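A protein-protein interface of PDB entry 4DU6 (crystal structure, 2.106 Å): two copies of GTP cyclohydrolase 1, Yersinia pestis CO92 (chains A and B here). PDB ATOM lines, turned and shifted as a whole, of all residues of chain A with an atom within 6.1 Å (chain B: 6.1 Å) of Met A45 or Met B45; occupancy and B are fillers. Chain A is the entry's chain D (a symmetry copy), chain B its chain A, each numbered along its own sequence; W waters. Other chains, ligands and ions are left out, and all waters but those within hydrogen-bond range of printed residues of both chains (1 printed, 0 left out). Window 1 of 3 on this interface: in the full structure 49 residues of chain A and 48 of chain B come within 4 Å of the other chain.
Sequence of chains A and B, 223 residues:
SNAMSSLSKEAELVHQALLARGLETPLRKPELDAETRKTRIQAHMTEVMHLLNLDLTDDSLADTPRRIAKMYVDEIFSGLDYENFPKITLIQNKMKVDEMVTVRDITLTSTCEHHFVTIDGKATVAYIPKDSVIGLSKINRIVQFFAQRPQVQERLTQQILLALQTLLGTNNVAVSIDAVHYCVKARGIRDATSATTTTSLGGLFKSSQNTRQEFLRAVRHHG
A ring nitrogen (ND1) of His B44 sits at hydrogen-bond distance from a ring nitrogen (ND1) of His A44 (2.9 Å).
SD of Met B45 lies close to SD of Met A45 (3.7 Å).
Among the printed residues, pairs that only touch across the chains: His A44 with Glu B47 (3.4 Å), Glu A47 with His B44 (3.4 Å), Ile A68 with Phe B116 (3.7 Å), His A44 with Val B48 (3.7 Å), Phe A116 with Met B49 (3.7 Å), Val A48 with His B44 (3.8 Å), Phe A116 with Ile B68 (3.8 Å), Phe A116 with Thr B64 (3.9 Å), Val A48 with Tyr B72 (3.9 Å), Thr A64 with Phe B116 (3.9 Å) and Met A49 with Phe B116 (3.97 Å).
Of the printed residues of chain B, Met A49 touches Phe B116.
Of the printed residues of chain A, Met B45 touches Met A45.
Printed residues of chain A within 4 Å of Glu B47: His A44.
Printed residues of chain A within 4 Å of Val B48: His A44 (3.7 Å).
Printed residues of chain A within 4 Å of Phe B116: Met A49 (3.97 Å), Thr A64 (3.9 Å) and Ile A68 (3.7 Å).
The nearest residue of chain B that does not touch Met A45 is Val B48 (4.2 Å).
The nearest printed residue of chain B that does not touch Thr A64 is Tyr B72 (9.1 Å).
Of the 17 printed residues of chain A, 8 touch a printed residue of chain B.
Printed residues of chain A that touch a printed residue of chain B: His A44, Met A45, Glu A47, Val A48, Met A49, Thr A64, Ile A68 and Phe A116.
Hydrophobic or aromatic side chains of chain A within 4 Å of the printed part of chain B: His A44, Met A45, Val A48, Met A49, Ile A68 and Phe A116.
Along chain A the printed residues that touch a printed residue of chain B span positions 44 to 116.
Of the 18 printed residues of chain B, 9 touch a printed residue of chain A.
Hydrophobic or aromatic side chains of chain B within 4 Å of the printed part of chain A: His B44, Met B45, Val B48, Met B49, Ile B68, Tyr B72 and Phe B116.
His A44 touches Val B48, and with the chains exchanged Val A48 touches His B44.
Val A48 touches Tyr B72, but with the chains exchanged Tyr A72 does not touch Val B48 (4.01 Å).
Met A49 touches Phe B116, and with the chains exchanged Phe A116 touches Met B49.
Ile A68 touches Phe B116, and with the chains exchanged Phe A116 touches Ile B68.
Positions printed for both chains: 40, 41, 42, 43, 44, 45, 46, 47, 48, 49, 50, 64, 65, 68, 69, 72 and 116.
Of the 13 pairs that touch across the chains among the printed residues, 12 have their exchanged pair printed and touching as well.
Water W1 bridges OE1 of Glu A47 (2.6 Å) and NE2 of His B44 (2.9 Å).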
ATOM      1  N   ARG A  40       5.994  29.114   0.550  1.00  0.00           N
ATOM      2  CA  ARG A  40       6.783  28.050  -0.046  1.00  0.00           C
ATOM      3  C   ARG A  40       8.242  28.529  -0.255  1.00  0.00           C
ATOM      4  O   ARG A  40       9.192  27.800   0.024  1.00  0.00           O
ATOM      5  CB  ARG A  40       6.163  27.585  -1.363  1.00  0.00           C
ATOM      6  CG  ARG A  40       4.766  26.901  -1.275  1.00  0.00           C
ATOM      7  CD  ARG A  40       4.785  25.525  -0.631  1.00  0.00           C
ATOM      8  NE  ARG A  40       3.431  24.996  -0.668  1.00  0.00           N
ATOM      9  CZ  ARG A  40       2.939  24.274  -1.672  1.00  0.00           C
ATOM     10  NH1 ARG A  40       3.706  23.946  -2.705  1.00  0.00           N
ATOM     11  NH2 ARG A  40       1.684  23.867  -1.636  1.00  0.00           N
ATOM     12  N   ILE A  41       8.409  29.768  -0.718  1.00  0.00           N
ATOM     13  CA  ILE A  41       9.749  30.342  -0.853  1.00  0.00           C
ATOM     14  C   ILE A  41      10.477  30.417   0.491  1.00  0.00           C
ATOM     15  O   ILE A  41      11.672  30.110   0.574  1.00  0.00           O
ATOM     16  CB  ILE A  41       9.766  31.685  -1.603  1.00  0.00           C
ATOM     17  CG1 ILE A  41       9.324  31.489  -3.048  1.00  0.00           C
ATOM     18  CG2 ILE A  41      11.186  32.279  -1.623  1.00  0.00           C
ATOM     19  CD1 ILE A  41       9.175  32.794  -3.823  1.00  0.00           C
ATOM     20  N   GLN A  42       9.765  30.790   1.543  1.00  0.00           N
ATOM     21  CA  GLN A  42      10.362  30.742   2.866  1.00  0.00           C
ATOM     22  C   GLN A  42      10.838  29.309   3.230  1.00  0.00           C
ATOM     23  O   GLN A  42      11.920  29.152   3.796  1.00  0.00           O
ATOM     24  CB  GLN A  42       9.385  31.275   3.912  1.00  0.00           C
ATOM     25  CG  GLN A  42       9.742  30.950   5.337  1.00  0.00           C
ATOM     26  CD  GLN A  42       8.767  31.584   6.302  1.00  0.00           C
ATOM     27  OE1 GLN A  42       7.923  32.381   5.896  1.00  0.00           O
ATOM     28  NE2 GLN A  42       8.858  31.220   7.582  1.00  0.00           N
ATOM     29  N   ALA A  43      10.048  28.277   2.886  1.00  0.00           N
ATOM     30  CA  ALA A  43      10.477  26.893   3.113  1.00  0.00           C
ATOM     31  C   ALA A  43      11.767  26.519   2.341  1.00  0.00           C
ATOM     32  O   ALA A  43      12.703  25.968   2.917  1.00  0.00           O
ATOM     33  CB  ALA A  43       9.315  25.856   2.837  1.00  0.00           C
ATOM     34  N   HIS A  44      11.835  26.835   1.054  1.00  0.00           N
ATOM     35  CA  HIS A  44      13.066  26.603   0.314  1.00  0.00           C
ATOM     36  C   HIS A  44      14.276  27.371   0.851  1.00  0.00           C
ATOM     37  O   HIS A  44      15.370  26.788   0.963  1.00  0.00           O
ATOM     38  CB  HIS A  44      12.875  26.856  -1.171  1.00  0.00           C
ATOM     39  CG  HIS A  44      11.944  25.880  -1.806  1.00  0.00           C
ATOM     40  ND1 HIS A  44      12.336  24.606  -2.147  1.00  0.00           N
ATOM     41  CD2 HIS A  44      10.642  25.976  -2.155  1.00  0.00           C
ATOM     42  CE1 HIS A  44      11.310  23.952  -2.662  1.00  0.00           C
ATOM     43  NE2 HIS A  44      10.273  24.767  -2.689  1.00  0.00           N
ATOM     44  N   MET A  45      14.087  28.640   1.214  1.00  0.00           N
ATOM     45  CA  MET A  45      15.217  29.453   1.684  1.00  0.00           C
ATOM     46  C   MET A  45      15.679  28.997   3.065  1.00  0.00           C
ATOM     47  O   MET A  45      16.882  29.008   3.366  1.00  0.00           O
ATOM     48  CB  MET A  45      14.917  30.963   1.666  1.00  0.00           C
ATOM     49  CG  MET A  45      14.723  31.549   0.259  1.00  0.00           C
ATOM     50  SD  MET A  45      16.010  31.078  -0.905  1.00  0.00           S
ATOM     51  CE  MET A  45      17.446  31.735   0.003  1.00  0.00           C
ATOM     52  N   THR A  46      14.715  28.564   3.878  1.00  0.00           N
ATOM     53  CA  THR A  46      14.991  27.885   5.137  1.00  0.00           C
ATOM     54  C   THR A  46      15.982  26.742   4.944  1.00  0.00           C
ATOM     55  O   THR A  46      16.942  26.644   5.679  1.00  0.00           O
ATOM     56  CB  THR A  46      13.701  27.320   5.753  1.00  0.00           C
ATOM     57  OG1 THR A  46      12.865  28.401   6.126  1.00  0.00           O
ATOM     58  CG2 THR A  46      14.014  26.491   6.992  1.00  0.00           C
ATOM     59  N   GLU A  47      15.750  25.899   3.942  1.00  0.00           N
ATOM     60  CA  GLU A  47      16.580  24.712   3.683  1.00  0.00           C
ATOM     61  C   GLU A  47      17.989  25.075   3.140  1.00  0.00           C
ATOM     62  O   GLU A  47      19.003  24.466   3.515  1.00  0.00           O
ATOM     63  CB  GLU A  47      15.860  23.816   2.703  1.00  0.00           C
ATOM     64  CG  GLU A  47      14.734  22.995   3.403  1.00  0.00           C
ATOM     65  CD  GLU A  47      15.299  22.211   4.576  1.00  0.00           C
ATOM     66  OE1 GLU A  47      16.078  21.251   4.336  1.00  0.00           O
ATOM     67  OE2 GLU A  47      14.992  22.573   5.734  1.00  0.00           O
ATOM     68  N   VAL A  48      18.017  26.048   2.233  1.00  0.00           N
ATOM     69  CA  VAL A  48      19.255  26.582   1.679  1.00  0.00           C
ATOM     70  C   VAL A  48      20.169  27.073   2.801  1.00  0.00           C
ATOM     71  O   VAL A  48      21.375  26.831   2.794  1.00  0.00           O
ATOM     72  CB  VAL A  48      18.972  27.753   0.724  1.00  0.00           C
ATOM     73  CG1 VAL A  48      20.322  28.541   0.362  1.00  0.00           C
ATOM     74  CG2 VAL A  48      18.242  27.249  -0.521  1.00  0.00           C
ATOM     75  N   MET A  49      19.581  27.734   3.782  1.00  0.00           N
ATOM     76  CA  MET A  49      20.358  28.290   4.865  1.00  0.00           C
ATOM     77  C   MET A  49      20.852  27.168   5.706  1.00  0.00           C
ATOM     78  O   MET A  49      21.999  27.174   6.134  1.00  0.00           O
ATOM     79  CB  MET A  49      19.531  29.264   5.708  1.00  0.00           C
ATOM     80  CG  MET A  49      19.417  30.650   5.098  1.00  0.00           C
ATOM     81  SD  MET A  49      18.453  31.734   6.181  1.00  0.00           S
ATOM     82  CE  MET A  49      19.747  32.376   7.267  1.00  0.00           C
ATOM     83  N   HIS A  50      19.982  26.179   5.926  1.00  0.00           N
ATOM     84  CA  HIS A  50      20.413  24.950   6.577  1.00  0.00           C
ATOM     85  C   HIS A  50      21.526  24.246   5.796  1.00  0.00           C
ATOM     86  O   HIS A  50      22.450  23.723   6.381  1.00  0.00           O
ATOM     87  CB  HIS A  50      19.263  23.978   6.781  1.00  0.00           C
ATOM     88  CG  HIS A  50      19.672  22.737   7.500  1.00  0.00           C
ATOM     89  ND1 HIS A  50      19.919  21.542   6.848  1.00  0.00           N
ATOM     90  CD2 HIS A  50      19.890  22.502   8.813  1.00  0.00           C
ATOM     91  CE1 HIS A  50      20.272  20.628   7.731  1.00  0.00           C
ATOM     92  NE2 HIS A  50      20.252  21.179   8.931  1.00  0.00           N
ATOM     93  N   THR A  64      15.206  35.104   8.763  1.00  0.00           N
ATOM     94  CA  THR A  64      15.721  35.403   7.425  1.00  0.00           C
ATOM     95  C   THR A  64      14.965  34.768   6.258  1.00  0.00           C
ATOM     96  O   THR A  64      14.646  35.461   5.309  1.00  0.00           O
ATOM     97  CB  THR A  64      17.251  35.170   7.315  1.00  0.00           C
ATOM     98  OG1 THR A  64      17.907  36.034   8.245  1.00  0.00           O
ATOM     99  CG2 THR A  64      17.758  35.460   5.904  1.00  0.00           C
ATOM    100  N   PRO A  65      14.647  33.460   6.329  1.00  0.00           N
ATOM    101  CA  PRO A  65      13.820  32.863   5.266  1.00  0.00           C
ATOM    102  C   PRO A  65      12.536  33.661   4.975  1.00  0.00           C
ATOM    103  O   PRO A  65      12.228  33.889   3.812  1.00  0.00           O
ATOM    104  CB  PRO A  65      13.483  31.479   5.829  1.00  0.00           C
ATOM    105  CG  PRO A  65      14.685  31.171   6.670  1.00  0.00           C
ATOM    106  CD  PRO A  65      15.067  32.455   7.317  1.00  0.00           C
ATOM    107  N   ILE A  68      13.420  37.009   3.196  1.00  0.00           N
ATOM    108  CA  ILE A  68      13.808  36.894   1.813  1.00  0.00           C
ATOM    109  C   ILE A  68      12.570  36.687   0.963  1.00  0.00           C
ATOM    110  O   ILE A  68      12.411  37.310  -0.087  1.00  0.00           O
ATOM    111  CB  ILE A  68      14.830  35.750   1.571  1.00  0.00           C
ATOM    112  CG1 ILE A  68      16.216  36.157   2.097  1.00  0.00           C
ATOM    113  CG2 ILE A  68      14.968  35.461   0.098  1.00  0.00           C
ATOM    114  CD1 ILE A  68      17.122  34.960   2.351  1.00  0.00           C
ATOM    115  N   ALA A  69      11.679  35.824   1.445  1.00  0.00           N
ATOM    116  CA  ALA A  69      10.525  35.423   0.680  1.00  0.00           C
ATOM    117  C   ALA A  69       9.704  36.654   0.430  1.00  0.00           C
ATOM    118  O   ALA A  69       9.269  36.900  -0.697  1.00  0.00           O
ATOM    119  CB  ALA A  69       9.676  34.320   1.459  1.00  0.00           C
ATOM    120  N   TYR A  72      11.598  38.936  -2.169  1.00  0.00           N
ATOM    121  CA  TYR A  72      11.441  38.473  -3.538  1.00  0.00           C
ATOM    122  C   TYR A  72      10.072  38.838  -4.113  1.00  0.00           C
ATOM    123  O   TYR A  72      10.003  39.587  -5.085  1.00  0.00           O
ATOM    124  CB  TYR A  72      11.685  36.959  -3.680  1.00  0.00           C
ATOM    125  CG  TYR A  72      13.142  36.546  -3.574  1.00  0.00           C
ATOM    126  CD1 TYR A  72      14.165  37.503  -3.480  1.00  0.00           C
ATOM    127  CD2 TYR A  72      13.496  35.207  -3.561  1.00  0.00           C
ATOM    128  CE1 TYR A  72      15.502  37.116  -3.382  1.00  0.00           C
ATOM    129  CE2 TYR A  72      14.827  34.815  -3.472  1.00  0.00           C
ATOM    130  CZ  TYR A  72      15.828  35.778  -3.379  1.00  0.00           C
ATOM    131  OH  TYR A  72      17.143  35.370  -3.269  1.00  0.00           O
ATOM    132  N   PHE A 116      21.384  36.450  -9.337  1.00  0.00           N
ATOM    133  CA  PHE A 116      20.435  36.950  -8.320  1.00  0.00           C
ATOM    134  C   PHE A 116      21.089  37.893  -7.319  1.00  0.00           C
ATOM    135  O   PHE A 116      20.830  37.864  -6.115  1.00  0.00           O
ATOM    136  CB  PHE A 116      19.661  35.803  -7.640  1.00  0.00           C
ATOM    137  CG  PHE A 116      18.357  35.501  -8.297  1.00  0.00           C
ATOM    138  CD1 PHE A 116      18.257  35.487  -9.674  1.00  0.00           C
ATOM    139  CD2 PHE A 116      17.233  35.230  -7.540  1.00  0.00           C
ATOM    140  CE1 PHE A 116      17.047  35.202 -10.286  1.00  0.00           C
ATOM    141  CE2 PHE A 116      16.010  34.907  -8.148  1.00  0.00           C
ATOM    142  CZ  PHE A 116      15.912  34.901  -9.517  1.00  0.00           C
ATOM    143  N   ARG B  40      21.854  20.254  -3.927  1.00  0.00           N
ATOM    144  CA  ARG B  40      20.577  20.429  -3.235  1.00  0.00           C
ATOM    145  C   ARG B  40      20.135  21.881  -3.182  1.00  0.00           C
ATOM    146  O   ARG B  40      18.933  22.170  -3.243  1.00  0.00           O
ATOM    147  CB  ARG B  40      20.674  19.887  -1.816  1.00  0.00           C
ATOM    148  CG  ARG B  40      20.723  18.383  -1.754  1.00  0.00           C
ATOM    149  CD  ARG B  40      21.189  17.923  -0.406  1.00  0.00           C
ATOM    150  NE  ARG B  40      21.323  16.483  -0.408  1.00  0.00           N
ATOM    151  CZ  ARG B  40      20.455  15.656   0.163  1.00  0.00           C
ATOM    152  NH1 ARG B  40      19.400  16.143   0.789  1.00  0.00           N
ATOM    153  NH2 ARG B  40      20.658  14.358   0.109  1.00  0.00           N
ATOM    154  N   ILE B  41      21.102  22.794  -3.050  1.00  0.00           N
ATOM    155  CA  ILE B  41      20.780  24.209  -3.053  1.00  0.00           C
ATOM    156  C   ILE B  41      20.289  24.584  -4.442  1.00  0.00           C
ATOM    157  O   ILE B  41      19.326  25.335  -4.569  1.00  0.00           O
ATOM    158  CB  ILE B  41      21.940  25.095  -2.578  1.00  0.00           C
ATOM    159  CG1 ILE B  41      22.146  24.921  -1.075  1.00  0.00           C
ATOM    160  CG2 ILE B  41      21.674  26.588  -2.877  1.00  0.00           C
ATOM    161  CD1 ILE B  41      23.350  25.755  -0.562  1.00  0.00           C
ATOM    162  N   GLN B  42      20.914  24.012  -5.466  1.00  0.00           N
ATOM    163  CA  GLN B  42      20.454  24.187  -6.835  1.00  0.00           C
ATOM    164  C   GLN B  42      19.015  23.694  -7.003  1.00  0.00           C
ATOM    165  O   GLN B  42      18.219  24.333  -7.683  1.00  0.00           O
ATOM    166  CB  GLN B  42      21.360  23.443  -7.816  1.00  0.00           C
ATOM    167  CG  GLN B  42      20.897  23.525  -9.263  1.00  0.00           C
ATOM    168  CD  GLN B  42      21.817  22.777 -10.210  1.00  0.00           C
ATOM    169  OE1 GLN B  42      22.961  22.483  -9.878  1.00  0.00           O
ATOM    170  NE2 GLN B  42      21.321  22.480 -11.401  1.00  0.00           N
ATOM    171  N   ALA B  43      18.669  22.589  -6.354  1.00  0.00           N
ATOM    172  CA  ALA B  43      17.297  22.096  -6.441  1.00  0.00           C
ATOM    173  C   ALA B  43      16.317  23.046  -5.777  1.00  0.00           C
ATOM    174  O   ALA B  43      15.313  23.419  -6.369  1.00  0.00           O
ATOM    175  CB  ALA B  43      17.139  20.619  -5.866  1.00  0.00           C
ATOM    176  N   HIS B  44      16.605  23.438  -4.545  1.00  0.00           N
ATOM    177  CA  HIS B  44      15.770  24.435  -3.872  1.00  0.00           C
ATOM    178  C   HIS B  44      15.644  25.753  -4.647  1.00  0.00           C
ATOM    179  O   HIS B  44      14.560  26.341  -4.693  1.00  0.00           O
ATOM    180  CB  HIS B  44      16.269  24.703  -2.458  1.00  0.00           C
ATOM    181  CG  HIS B  44      15.992  23.575  -1.514  1.00  0.00           C
ATOM    182  ND1 HIS B  44      14.713  23.184  -1.199  1.00  0.00           N
ATOM    183  CD2 HIS B  44      16.820  22.775  -0.806  1.00  0.00           C
ATOM    184  CE1 HIS B  44      14.764  22.169  -0.355  1.00  0.00           C
ATOM    185  NE2 HIS B  44      16.029  21.904  -0.095  1.00  0.00           N
ATOM    186  N   MET B  45      16.722  26.206  -5.284  1.00  0.00           N
ATOM    187  CA  MET B  45      16.657  27.520  -5.938  1.00  0.00           C
ATOM    188  C   MET B  45      15.919  27.411  -7.257  1.00  0.00           C
ATOM    189  O   MET B  45      15.362  28.408  -7.739  1.00  0.00           O
ATOM    190  CB  MET B  45      18.036  28.140  -6.167  1.00  0.00           C
ATOM    191  CG  MET B  45      18.736  28.545  -4.901  1.00  0.00           C
ATOM    192  SD  MET B  45      17.722  29.582  -3.814  1.00  0.00           S
ATOM    193  CE  MET B  45      17.647  31.125  -4.713  1.00  0.00           C
ATOM    194  N   THR B  46      15.959  26.214  -7.845  1.00  0.00           N
ATOM    195  CA  THR B  46      15.162  25.928  -9.022  1.00  0.00           C
ATOM    196  C   THR B  46      13.668  26.133  -8.689  1.00  0.00           C
ATOM    197  O   THR B  46      12.940  26.784  -9.437  1.00  0.00           O
ATOM    198  CB  THR B  46      15.404  24.476  -9.508  1.00  0.00           C
ATOM    199  OG1 THR B  46      16.751  24.350  -9.980  1.00  0.00           O
ATOM    200  CG2 THR B  46      14.464  24.117 -10.637  1.00  0.00           C
ATOM    201  N   GLU B  47      13.224  25.600  -7.551  1.00  0.00           N
ATOM    202  CA  GLU B  47      11.826  25.762  -7.101  1.00  0.00           C
ATOM    203  C   GLU B  47      11.406  27.209  -6.807  1.00  0.00           C
ATOM    204  O   GLU B  47      10.288  27.610  -7.154  1.00  0.00           O
ATOM    205  CB  GLU B  47      11.536  24.880  -5.879  1.00  0.00           C
ATOM    206  CG  GLU B  47      11.730  23.404  -6.162  1.00  0.00           C
ATOM    207  CD  GLU B  47      10.985  22.968  -7.410  1.00  0.00           C
ATOM    208  OE1 GLU B  47       9.734  23.087  -7.410  1.00  0.00           O
ATOM    209  OE2 GLU B  47      11.654  22.523  -8.386  1.00  0.00           O
ATOM    210  N   VAL B  48      12.301  27.962  -6.154  1.00  0.00           N
ATOM    211  CA  VAL B  48      12.096  29.384  -5.890  1.00  0.00           C
ATOM    212  C   VAL B  48      11.807  30.153  -7.178  1.00  0.00           C
ATOM    213  O   VAL B  48      10.921  30.997  -7.224  1.00  0.00           O
ATOM    214  CB  VAL B  48      13.320  30.018  -5.166  1.00  0.00           C
ATOM    215  CG1 VAL B  48      13.225  31.536  -5.156  1.00  0.00           C
ATOM    216  CG2 VAL B  48      13.404  29.487  -3.746  1.00  0.00           C
ATOM    217  N   MET B  49      12.546  29.845  -8.230  1.00  0.00           N
ATOM    218  CA  MET B  49      12.316  30.486  -9.511  1.00  0.00           C
ATOM    219  C   MET B  49      10.947  30.150 -10.080  1.00  0.00           C
ATOM    220  O   MET B  49      10.199  31.044 -10.466  1.00  0.00           O
ATOM    221  CB  MET B  49      13.467  30.164 -10.456  1.00  0.00           C
ATOM    222  CG  MET B  49      14.750  30.736  -9.879  1.00  0.00           C
ATOM    223  SD  MET B  49      16.148  30.909 -10.974  1.00  0.00           S
ATOM    224  CE  MET B  49      15.540  32.183 -12.058  1.00  0.00           C
ATOM    225  N   HIS B  50      10.598  28.866 -10.078  1.00  0.00           N
ATOM    226  CA  HIS B  50       9.244  28.447 -10.428  1.00  0.00           C
ATOM    227  C   HIS B  50       8.205  29.218  -9.633  1.00  0.00           C
ATOM    228  O   HIS B  50       7.248  29.741 -10.192  1.00  0.00           O
ATOM    229  CB  HIS B  50       9.058  26.959 -10.200  1.00  0.00           C
ATOM    230  CG  HIS B  50       9.763  26.108 -11.206  1.00  0.00           C
ATOM    231  ND1 HIS B  50      10.228  24.842 -10.918  1.00  0.00           N
ATOM    232  CD2 HIS B  50      10.096  26.345 -12.496  1.00  0.00           C
ATOM    233  CE1 HIS B  50      10.814  24.335 -11.987  1.00  0.00           C
ATOM    234  NE2 HIS B  50      10.734  25.222 -12.963  1.00  0.00           N
ATOM    235  N   LEU B  56      12.015  29.080 -16.688  1.00  0.00           N
ATOM    236  CA  LEU B  56      13.359  28.530 -16.653  1.00  0.00           C
ATOM    237  C   LEU B  56      13.892  27.970 -17.988  1.00  0.00           C
ATOM    238  O   LEU B  56      15.103  27.755 -18.130  1.00  0.00           O
ATOM    239  CB  LEU B  56      13.446  27.487 -15.550  1.00  0.00           C
ATOM    240  CG  LEU B  56      13.729  28.079 -14.177  1.00  0.00           C
ATOM    241  CD1 LEU B  56      13.638  26.997 -13.141  1.00  0.00           C
ATOM    242  CD2 LEU B  56      15.107  28.693 -14.163  1.00  0.00           C
ATOM    243  N   THR B  64      20.691  29.520 -13.898  1.00  0.00           N
ATOM    244  CA  THR B  64      20.685  30.390 -12.721  1.00  0.00           C
ATOM    245  C   THR B  64      20.717  29.671 -11.381  1.00  0.00           C
ATOM    246  O   THR B  64      21.504  30.018 -10.527  1.00  0.00           O
ATOM    247  CB  THR B  64      19.579  31.465 -12.804  1.00  0.00           C
ATOM    248  OG1 THR B  64      19.929  32.353 -13.860  1.00  0.00           O
ATOM    249  CG2 THR B  64      19.490  32.292 -11.520  1.00  0.00           C
ATOM    250  N   PRO B  65      19.912  28.608 -11.211  1.00  0.00           N
ATOM    251  CA  PRO B  65      20.005  27.907  -9.919  1.00  0.00           C
ATOM    252  C   PRO B  65      21.381  27.281  -9.607  1.00  0.00           C
ATOM    253  O   PRO B  65      21.801  27.291  -8.452  1.00  0.00           O
ATOM    254  CB  PRO B  65      18.950  26.816 -10.063  1.00  0.00           C
ATOM    255  CG  PRO B  65      17.947  27.403 -10.943  1.00  0.00           C
ATOM    256  CD  PRO B  65      18.661  28.287 -11.920  1.00  0.00           C
ATOM    257  N   ILE B  68      23.774  30.202  -8.750  1.00  0.00           N
ATOM    258  CA  ILE B  68      23.509  30.643  -7.391  1.00  0.00           C
ATOM    259  C   ILE B  68      24.064  29.692  -6.340  1.00  0.00           C
ATOM    260  O   ILE B  68      24.669  30.133  -5.369  1.00  0.00           O
ATOM    261  CB  ILE B  68      21.985  30.838  -7.153  1.00  0.00           C
ATOM    262  CG1 ILE B  68      21.485  32.037  -7.965  1.00  0.00           C
ATOM    263  CG2 ILE B  68      21.668  31.100  -5.690  1.00  0.00           C
ATOM    264  CD1 ILE B  68      19.948  32.070  -7.980  1.00  0.00           C
ATOM    265  N   ALA B  69      23.871  28.392  -6.534  1.00  0.00           N
ATOM    266  CA  ALA B  69      24.376  27.397  -5.601  1.00  0.00           C
ATOM    267  C   ALA B  69      25.894  27.455  -5.543  1.00  0.00           C
ATOM    268  O   ALA B  69      26.480  27.432  -4.454  1.00  0.00           O
ATOM    269  CB  ALA B  69      23.895  25.944  -5.997  1.00  0.00           C
ATOM    270  N   TYR B  72      26.871  30.747  -3.647  1.00  0.00           N
ATOM    271  CA  TYR B  72      26.691  30.719  -2.202  1.00  0.00           C
ATOM    272  C   TYR B  72      27.754  29.886  -1.514  1.00  0.00           C
ATOM    273  O   TYR B  72      28.438  30.375  -0.618  1.00  0.00           O
ATOM    274  CB  TYR B  72      25.337  30.123  -1.838  1.00  0.00           C
ATOM    275  CG  TYR B  72      24.163  31.052  -1.992  1.00  0.00           C
ATOM    276  CD1 TYR B  72      24.322  32.370  -2.408  1.00  0.00           C
ATOM    277  CD2 TYR B  72      22.883  30.594  -1.738  1.00  0.00           C
ATOM    278  CE1 TYR B  72      23.219  33.227  -2.539  1.00  0.00           C
ATOM    279  CE2 TYR B  72      21.785  31.434  -1.863  1.00  0.00           C
ATOM    280  CZ  TYR B  72      21.943  32.736  -2.274  1.00  0.00           C
ATOM    281  OH  TYR B  72      20.807  33.534  -2.401  1.00  0.00           O
ATOM    282  N   PHE B 116      19.978  38.707   2.971  1.00  0.00           N
ATOM    283  CA  PHE B 116      20.813  38.076   1.943  1.00  0.00           C
ATOM    284  C   PHE B 116      20.988  38.950   0.689  1.00  0.00           C
ATOM    285  O   PHE B 116      20.825  38.487  -0.431  1.00  0.00           O
ATOM    286  CB  PHE B 116      20.276  36.668   1.597  1.00  0.00           C
ATOM    287  CG  PHE B 116      20.868  35.573   2.442  1.00  0.00           C
ATOM    288  CD1 PHE B 116      21.039  35.747   3.804  1.00  0.00           C
ATOM    289  CD2 PHE B 116      21.247  34.365   1.870  1.00  0.00           C
ATOM    290  CE1 PHE B 116      21.566  34.714   4.584  1.00  0.00           C
ATOM    291  CE2 PHE B 116      21.772  33.346   2.636  1.00  0.00           C
ATOM    292  CZ  PHE B 116      21.937  33.516   4.000  1.00  0.00           C
HETATM  293  O   HOH W   1      16.697  20.182   2.087  1.00  0.00           O
